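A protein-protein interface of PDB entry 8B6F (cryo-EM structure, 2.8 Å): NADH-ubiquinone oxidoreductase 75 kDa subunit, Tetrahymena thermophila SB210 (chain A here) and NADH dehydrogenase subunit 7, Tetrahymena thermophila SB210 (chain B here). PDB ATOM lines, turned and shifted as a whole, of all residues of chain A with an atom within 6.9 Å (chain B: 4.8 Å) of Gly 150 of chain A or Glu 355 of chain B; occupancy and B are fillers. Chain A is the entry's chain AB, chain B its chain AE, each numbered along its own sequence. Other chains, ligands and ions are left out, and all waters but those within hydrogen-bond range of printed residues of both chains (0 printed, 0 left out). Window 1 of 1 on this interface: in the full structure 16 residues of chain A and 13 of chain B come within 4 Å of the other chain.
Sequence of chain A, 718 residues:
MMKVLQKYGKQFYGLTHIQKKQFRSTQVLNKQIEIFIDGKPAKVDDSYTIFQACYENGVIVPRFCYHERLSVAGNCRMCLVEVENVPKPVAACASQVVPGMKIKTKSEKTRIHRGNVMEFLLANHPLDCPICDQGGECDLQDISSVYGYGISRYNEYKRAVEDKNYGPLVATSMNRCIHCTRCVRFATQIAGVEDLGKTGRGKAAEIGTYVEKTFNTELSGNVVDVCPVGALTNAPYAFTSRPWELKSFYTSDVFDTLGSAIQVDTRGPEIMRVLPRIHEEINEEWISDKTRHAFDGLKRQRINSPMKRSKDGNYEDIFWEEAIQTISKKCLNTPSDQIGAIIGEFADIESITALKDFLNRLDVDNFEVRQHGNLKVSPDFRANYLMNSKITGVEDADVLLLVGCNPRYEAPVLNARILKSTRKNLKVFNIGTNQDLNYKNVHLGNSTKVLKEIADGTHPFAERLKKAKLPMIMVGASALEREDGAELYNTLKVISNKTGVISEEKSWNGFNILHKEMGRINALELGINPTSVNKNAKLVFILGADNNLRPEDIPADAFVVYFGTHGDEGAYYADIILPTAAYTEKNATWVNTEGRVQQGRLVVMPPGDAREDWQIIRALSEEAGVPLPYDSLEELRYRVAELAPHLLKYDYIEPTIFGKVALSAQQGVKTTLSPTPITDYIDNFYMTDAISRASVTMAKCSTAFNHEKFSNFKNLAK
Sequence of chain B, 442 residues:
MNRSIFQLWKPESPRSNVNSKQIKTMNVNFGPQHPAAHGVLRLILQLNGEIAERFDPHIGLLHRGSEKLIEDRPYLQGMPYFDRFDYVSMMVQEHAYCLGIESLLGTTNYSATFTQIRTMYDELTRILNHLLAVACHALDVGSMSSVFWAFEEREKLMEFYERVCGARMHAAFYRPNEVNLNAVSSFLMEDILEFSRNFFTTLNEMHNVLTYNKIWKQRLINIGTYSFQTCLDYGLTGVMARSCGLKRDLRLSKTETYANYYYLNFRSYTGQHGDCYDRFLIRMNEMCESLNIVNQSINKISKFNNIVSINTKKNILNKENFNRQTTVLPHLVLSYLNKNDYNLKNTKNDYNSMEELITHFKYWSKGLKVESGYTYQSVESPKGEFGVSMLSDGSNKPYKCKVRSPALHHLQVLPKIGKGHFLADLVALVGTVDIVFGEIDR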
ATOM      1  N   GLY A 115     -14.526  -2.498 -25.189  1.00  0.00           N
ATOM      2  CA  GLY A 115     -14.206  -3.750 -24.528  1.00  0.00           C
ATOM      3  C   GLY A 115     -15.194  -4.109 -23.436  1.00  0.00           C
ATOM      4  O   GLY A 115     -15.597  -5.267 -23.308  1.00  0.00           O
ATOM      5  N   MET A 118     -18.508  -5.185 -25.077  1.00  0.00           N
ATOM      6  CA  MET A 118     -18.363  -6.491 -25.708  1.00  0.00           C
ATOM      7  C   MET A 118     -18.286  -7.597 -24.666  1.00  0.00           C
ATOM      8  O   MET A 118     -18.861  -8.675 -24.855  1.00  0.00           O
ATOM      9  CB  MET A 118     -17.123  -6.508 -26.601  1.00  0.00           C
ATOM     10  CG  MET A 118     -16.854  -7.850 -27.268  1.00  0.00           C
ATOM     11  SD  MET A 118     -18.291  -8.532 -28.118  1.00  0.00           S
ATOM     12  CE  MET A 118     -18.725  -7.174 -29.201  1.00  0.00           C
ATOM     13  N   GLU A 119     -17.584  -7.352 -23.558  1.00  0.00           N
ATOM     14  CA  GLU A 119     -17.517  -8.351 -22.499  1.00  0.00           C
ATOM     15  C   GLU A 119     -18.898  -8.621 -21.919  1.00  0.00           C
ATOM     16  O   GLU A 119     -19.261  -9.777 -21.673  1.00  0.00           O
ATOM     17  CB  GLU A 119     -16.558  -7.888 -21.404  1.00  0.00           C
ATOM     18  CG  GLU A 119     -16.390  -8.885 -20.270  1.00  0.00           C
ATOM     19  CD  GLU A 119     -15.448  -8.386 -19.194  1.00  0.00           C
ATOM     20  OE1 GLU A 119     -15.128  -7.180 -19.195  1.00  0.00           O
ATOM     21  OE2 GLU A 119     -15.024  -9.200 -18.347  1.00  0.00           O
ATOM     22  N   PHE A 120     -19.679  -7.567 -21.680  1.00  0.00           N
ATOM     23  CA  PHE A 120     -21.032  -7.753 -21.172  1.00  0.00           C
ATOM     24  C   PHE A 120     -21.893  -8.514 -22.172  1.00  0.00           C
ATOM     25  O   PHE A 120     -22.678  -9.387 -21.788  1.00  0.00           O
ATOM     26  CB  PHE A 120     -21.656  -6.398 -20.836  1.00  0.00           C
ATOM     27  CG  PHE A 120     -21.093  -5.763 -19.593  1.00  0.00           C
ATOM     28  CD1 PHE A 120     -20.960  -6.493 -18.422  1.00  0.00           C
ATOM     29  CD2 PHE A 120     -20.685  -4.440 -19.600  1.00  0.00           C
ATOM     30  CE1 PHE A 120     -20.440  -5.915 -17.283  1.00  0.00           C
ATOM     31  CE2 PHE A 120     -20.164  -3.857 -18.463  1.00  0.00           C
ATOM     32  CZ  PHE A 120     -20.042  -4.595 -17.303  1.00  0.00           C
ATOM     33  N   LEU A 122     -20.870 -10.715 -24.438  1.00  0.00           N
ATOM     34  CA  LEU A 122     -20.450 -12.106 -24.550  1.00  0.00           C
ATOM     35  C   LEU A 122     -20.742 -12.891 -23.282  1.00  0.00           C
ATOM     36  O   LEU A 122     -20.882 -14.116 -23.345  1.00  0.00           O
ATOM     37  CB  LEU A 122     -18.965 -12.181 -24.897  1.00  0.00           C
ATOM     38  CG  LEU A 122     -18.604 -11.602 -26.269  1.00  0.00           C
ATOM     39  CD1 LEU A 122     -17.109 -11.645 -26.479  1.00  0.00           C
ATOM     40  CD2 LEU A 122     -19.315 -12.336 -27.396  1.00  0.00           C
ATOM     41  N   LEU A 127     -21.636 -21.020 -26.269  1.00  0.00           N
ATOM     42  CA  LEU A 127     -20.502 -21.397 -27.109  1.00  0.00           C
ATOM     43  C   LEU A 127     -21.003 -22.248 -28.277  1.00  0.00           C
ATOM     44  O   LEU A 127     -20.798 -23.460 -28.345  1.00  0.00           O
ATOM     45  CB  LEU A 127     -19.468 -22.143 -26.273  1.00  0.00           C
ATOM     46  CG  LEU A 127     -19.029 -21.490 -24.958  1.00  0.00           C
ATOM     47  CD1 LEU A 127     -17.820 -22.208 -24.382  1.00  0.00           C
ATOM     48  CD2 LEU A 127     -18.716 -20.027 -25.157  1.00  0.00           C
ATOM     49  N   SER A 144     -16.059  -8.492 -31.845  1.00  0.00           N
ATOM     50  CA  SER A 144     -15.271  -9.020 -30.740  1.00  0.00           C
ATOM     51  C   SER A 144     -13.807  -9.165 -31.128  1.00  0.00           C
ATOM     52  O   SER A 144     -12.921  -8.974 -30.288  1.00  0.00           O
ATOM     53  CB  SER A 144     -15.834 -10.367 -30.289  1.00  0.00           C
ATOM     54  OG  SER A 144     -15.043 -10.929 -29.257  1.00  0.00           O
ATOM     55  N   SER A 145     -13.532  -9.513 -32.385  1.00  0.00           N
ATOM     56  CA  SER A 145     -12.148  -9.658 -32.821  1.00  0.00           C
ATOM     57  C   SER A 145     -11.473  -8.303 -33.002  1.00  0.00           C
ATOM     58  O   SER A 145     -10.285  -8.152 -32.695  1.00  0.00           O
ATOM     59  CB  SER A 145     -12.093 -10.453 -34.126  1.00  0.00           C
ATOM     60  OG  SER A 145     -12.550 -11.780 -33.933  1.00  0.00           O
ATOM     61  N   GLY A 148     -13.292  -5.617 -29.178  1.00  0.00           N
ATOM     62  CA  GLY A 148     -13.341  -6.121 -27.824  1.00  0.00           C
ATOM     63  C   GLY A 148     -12.044  -6.784 -27.397  1.00  0.00           C
ATOM     64  O   GLY A 148     -11.111  -6.961 -28.178  1.00  0.00           O
ATOM     65  N   TYR A 149     -11.996  -7.148 -26.118  1.00  0.00           N
ATOM     66  CA  TYR A 149     -10.838  -7.842 -25.578  1.00  0.00           C
ATOM     67  C   TYR A 149     -10.752  -9.249 -26.166  1.00  0.00           C
ATOM     68  O   TYR A 149     -11.697  -9.762 -26.772  1.00  0.00           O
ATOM     69  CB  TYR A 149     -10.911  -7.911 -24.053  1.00  0.00           C
ATOM     70  CG  TYR A 149     -11.081  -6.575 -23.368  1.00  0.00           C
ATOM     71  CD1 TYR A 149     -10.114  -5.584 -23.482  1.00  0.00           C
ATOM     72  CD2 TYR A 149     -12.198  -6.310 -22.588  1.00  0.00           C
ATOM     73  CE1 TYR A 149     -10.263  -4.364 -22.848  1.00  0.00           C
ATOM     74  CE2 TYR A 149     -12.356  -5.095 -21.951  1.00  0.00           C
ATOM     75  CZ  TYR A 149     -11.386  -4.127 -22.085  1.00  0.00           C
ATOM     76  OH  TYR A 149     -11.539  -2.918 -21.450  1.00  0.00           O
ATOM     77  N   GLY A 150      -9.595  -9.877 -25.983  1.00  0.00           N
ATOM     78  CA  GLY A 150      -9.347 -11.179 -26.570  1.00  0.00           C
ATOM     79  C   GLY A 150      -9.629 -12.351 -25.653  1.00  0.00           C
ATOM     80  O   GLY A 150      -9.589 -13.503 -26.095  1.00  0.00           O
ATOM     81  N   ILE A 151      -9.913 -12.082 -24.380  1.00  0.00           N
ATOM     82  CA  ILE A 151     -10.162 -13.131 -23.399  1.00  0.00           C
ATOM     83  C   ILE A 151     -11.295 -12.685 -22.485  1.00  0.00           C
ATOM     84  O   ILE A 151     -11.500 -11.490 -22.255  1.00  0.00           O
ATOM     85  CB  ILE A 151      -8.889 -13.465 -22.588  1.00  0.00           C
ATOM     86  CG1 ILE A 151      -7.811 -14.010 -23.530  1.00  0.00           C
ATOM     87  CG2 ILE A 151      -9.200 -14.464 -21.474  1.00  0.00           C
ATOM     88  CD1 ILE A 151      -6.529 -14.446 -22.852  1.00  0.00           C
ATOM     89  N   SER A 152     -12.037 -13.661 -21.970  1.00  0.00           N
ATOM     90  CA  SER A 152     -13.198 -13.416 -21.131  1.00  0.00           C
ATOM     91  C   SER A 152     -12.901 -13.807 -19.689  1.00  0.00           C
ATOM     92  O   SER A 152     -12.098 -14.706 -19.424  1.00  0.00           O
ATOM     93  CB  SER A 152     -14.411 -14.199 -21.640  1.00  0.00           C
ATOM     94  OG  SER A 152     -15.572 -13.900 -20.882  1.00  0.00           O
ATOM     95  N   ARG A 153     -13.560 -13.116 -18.757  1.00  0.00           N
ATOM     96  CA  ARG A 153     -13.427 -13.400 -17.334  1.00  0.00           C
ATOM     97  C   ARG A 153     -14.627 -14.129 -16.751  1.00  0.00           C
ATOM     98  O   ARG A 153     -14.488 -14.785 -15.713  1.00  0.00           O
ATOM     99  CB  ARG A 153     -13.225 -12.102 -16.545  1.00  0.00           C
ATOM    100  CG  ARG A 153     -11.947 -11.372 -16.878  1.00  0.00           C
ATOM    101  CD  ARG A 153     -11.823 -10.087 -16.079  1.00  0.00           C
ATOM    102  NE  ARG A 153     -12.895  -9.147 -16.376  1.00  0.00           N
ATOM    103  CZ  ARG A 153     -12.970  -7.919 -15.882  1.00  0.00           C
ATOM    104  NH1 ARG A 153     -12.046  -7.446 -15.062  1.00  0.00           N
ATOM    105  NH2 ARG A 153     -13.998  -7.147 -16.219  1.00  0.00           N
ATOM    106  N   SER B 353     -14.388 -20.430 -22.700  1.00  0.00           N
ATOM    107  CA  SER B 353     -14.418 -18.980 -22.844  1.00  0.00           C
ATOM    108  C   SER B 353     -15.004 -18.614 -24.200  1.00  0.00           C
ATOM    109  O   SER B 353     -14.544 -19.106 -25.234  1.00  0.00           O
ATOM    110  CB  SER B 353     -13.013 -18.390 -22.689  1.00  0.00           C
ATOM    111  OG  SER B 353     -13.026 -16.985 -22.862  1.00  0.00           O
ATOM    112  N   MET B 354     -16.021 -17.747 -24.187  1.00  0.00           N
ATOM    113  CA  MET B 354     -16.655 -17.320 -25.432  1.00  0.00           C
ATOM    114  C   MET B 354     -15.672 -16.578 -26.325  1.00  0.00           C
ATOM    115  O   MET B 354     -15.634 -16.801 -27.540  1.00  0.00           O
ATOM    116  CB  MET B 354     -17.863 -16.436 -25.117  1.00  0.00           C
ATOM    117  CG  MET B 354     -18.682 -15.996 -26.329  1.00  0.00           C
ATOM    118  SD  MET B 354     -19.785 -17.264 -26.981  1.00  0.00           S
ATOM    119  CE  MET B 354     -18.795 -17.946 -28.306  1.00  0.00           C
ATOM    120  N   GLU B 355     -14.864 -15.692 -25.743  1.00  0.00           N
ATOM    121  CA  GLU B 355     -13.890 -14.950 -26.536  1.00  0.00           C
ATOM    122  C   GLU B 355     -12.846 -15.880 -27.135  1.00  0.00           C
ATOM    123  O   GLU B 355     -12.448 -15.715 -28.294  1.00  0.00           O
ATOM    124  CB  GLU B 355     -13.228 -13.871 -25.680  1.00  0.00           C
ATOM    125  CG  GLU B 355     -14.179 -12.756 -25.277  1.00  0.00           C
ATOM    126  CD  GLU B 355     -13.475 -11.592 -24.606  1.00  0.00           C
ATOM    127  OE1 GLU B 355     -12.254 -11.434 -24.818  1.00  0.00           O
ATOM    128  OE2 GLU B 355     -14.142 -10.834 -23.870  1.00  0.00           O
ATOM    129  N   GLU B 356     -12.385 -16.864 -26.363  1.00  0.00           N
ATOM    130  CA  GLU B 356     -11.432 -17.828 -26.902  1.00  0.00           C
ATOM    131  C   GLU B 356     -12.050 -18.628 -28.040  1.00  0.00           C
ATOM    132  O   GLU B 356     -11.391 -18.890 -29.052  1.00  0.00           O
ATOM    133  CB  GLU B 356     -10.953 -18.768 -25.795  1.00  0.00           C
ATOM    134  CG  GLU B 356     -10.114 -18.091 -24.727  1.00  0.00           C
ATOM    135  CD  GLU B 356      -8.739 -17.698 -25.229  1.00  0.00           C
ATOM    136  OE1 GLU B 356      -8.451 -17.929 -26.422  1.00  0.00           O
ATOM    137  OE2 GLU B 356      -7.943 -17.163 -24.430  1.00  0.00           O
ATOM    138  N   LEU B 357     -13.312 -19.036 -27.891  1.00  0.00           N
ATOM    139  CA  LEU B 357     -13.970 -19.773 -28.963  1.00  0.00           C
ATOM    140  C   LEU B 357     -14.086 -18.924 -30.220  1.00  0.00           C
ATOM    141  O   LEU B 357     -13.847 -19.410 -31.332  1.00  0.00           O
ATOM    142  CB  LEU B 357     -15.354 -20.240 -28.517  1.00  0.00           C
ATOM    143  CG  LEU B 357     -16.104 -21.076 -29.558  1.00  0.00           C
ATOM    144  CD1 LEU B 357     -15.400 -22.401 -29.788  1.00  0.00           C
ATOM    145  CD2 LEU B 357     -17.521 -21.308 -29.129  1.00  0.00           C
ATOM    146  N   ILE B 358     -14.463 -17.653 -30.068  1.00  0.00           N
ATOM    147  CA  ILE B 358     -14.583 -16.781 -31.232  1.00  0.00           C
ATOM    148  C   ILE B 358     -13.227 -16.600 -31.895  1.00  0.00           C
ATOM    149  O   ILE B 358     -13.110 -16.642 -33.124  1.00  0.00           O
ATOM    150  CB  ILE B 358     -15.205 -15.432 -30.825  1.00  0.00           C
ATOM    151  CG1 ILE B 358     -16.675 -15.628 -30.446  1.00  0.00           C
ATOM    152  CG2 ILE B 358     -15.072 -14.414 -31.953  1.00  0.00           C
ATOM    153  CD1 ILE B 358     -17.350 -14.388 -29.897  1.00  0.00           C
ATOM    154  N   THR B 359     -12.181 -16.389 -31.095  1.00  0.00           N
ATOM    155  CA  THR B 359     -10.848 -16.231 -31.665  1.00  0.00           C
ATOM    156  C   THR B 359     -10.426 -17.491 -32.407  1.00  0.00           C
ATOM    157  O   THR B 359      -9.860 -17.416 -33.503  1.00  0.00           O
ATOM    158  CB  THR B 359      -9.844 -15.893 -30.564  1.00  0.00           C
ATOM    159  OG1 THR B 359     -10.206 -14.652 -29.945  1.00  0.00           O
ATOM    160  CG2 THR B 359      -8.436 -15.770 -31.130  1.00  0.00           C
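O of Tyr 149 of chain A sits close to OE1 of Glu 355 of chain B, at 2.6 Å.
The backbone NH of Ile 151 of chain A lies within hydrogen-bond range of the side-chain carboxylate of Glu 355 of chain B.
N of Gly 150 of chain A lies close to OE1 of Glu 355 of chain B, 3.3 Å away.
The backbone carbonyl oxygen (O) of Glu 355 of chain B sits at hydrogen-bond distance from the side-chain hydroxyl (OG1) of Thr 359 of chain B (3.0 Å).
Leu 122 of chain A touches Met 354 of chain B.
Leu 122 of chain A touches Glu 355 of chain B.
Leu 122 of chain A touches Ile 358 of chain B (CD2 to CD1, 3.8 Å).
CD2 of Leu 127 of chain A touches CA of Met 354 of chain B (3.4 Å).
CB of Leu 127 of chain A touches CD2 of Leu 357 of chain B, 3.6 Å away.
Ile 151 of chain A touches Glu 356 of chain B.
CB of Ser 152 of chain A touches OG of Ser 353 of chain B, 3.3 Å away.
Ser 152 of chain A touches Glu 355 of chain B.
Printed residues of chain B within 4 Å of Gly 150 of chain A: Glu 355.
Glu 355 of chain B touches five residues of chain A.
Of the printed residues of chain B, Ser 152 of chain A touches Ser 353 (3.3 Å) and Glu 355 (3.6 Å).
Of the printed residues of chain A, Met 354 of chain B touches Leu 122 and Leu 127.
Of the printed residues of chain B, Ile 151 of chain A touches Glu 355 (2.5 Å) and Glu 356 (3.3 Å).
Of the printed residues of chain A, Leu 357 of chain B touches Leu 127.
Gly 115 of chain A touches none of the printed residues of chain B.
The nearest printed residue of chain A that does not touch Ser 353 of chain B is Leu 127 of chain A (4.1 Å).
Of the 14 printed residues of chain A, 6 touch a printed residue of chain B.
Hydrophobic or aromatic side chains of chain A that line the printed part of chain B: Leu 122, Leu 127, Tyr 149 and Ile 151.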
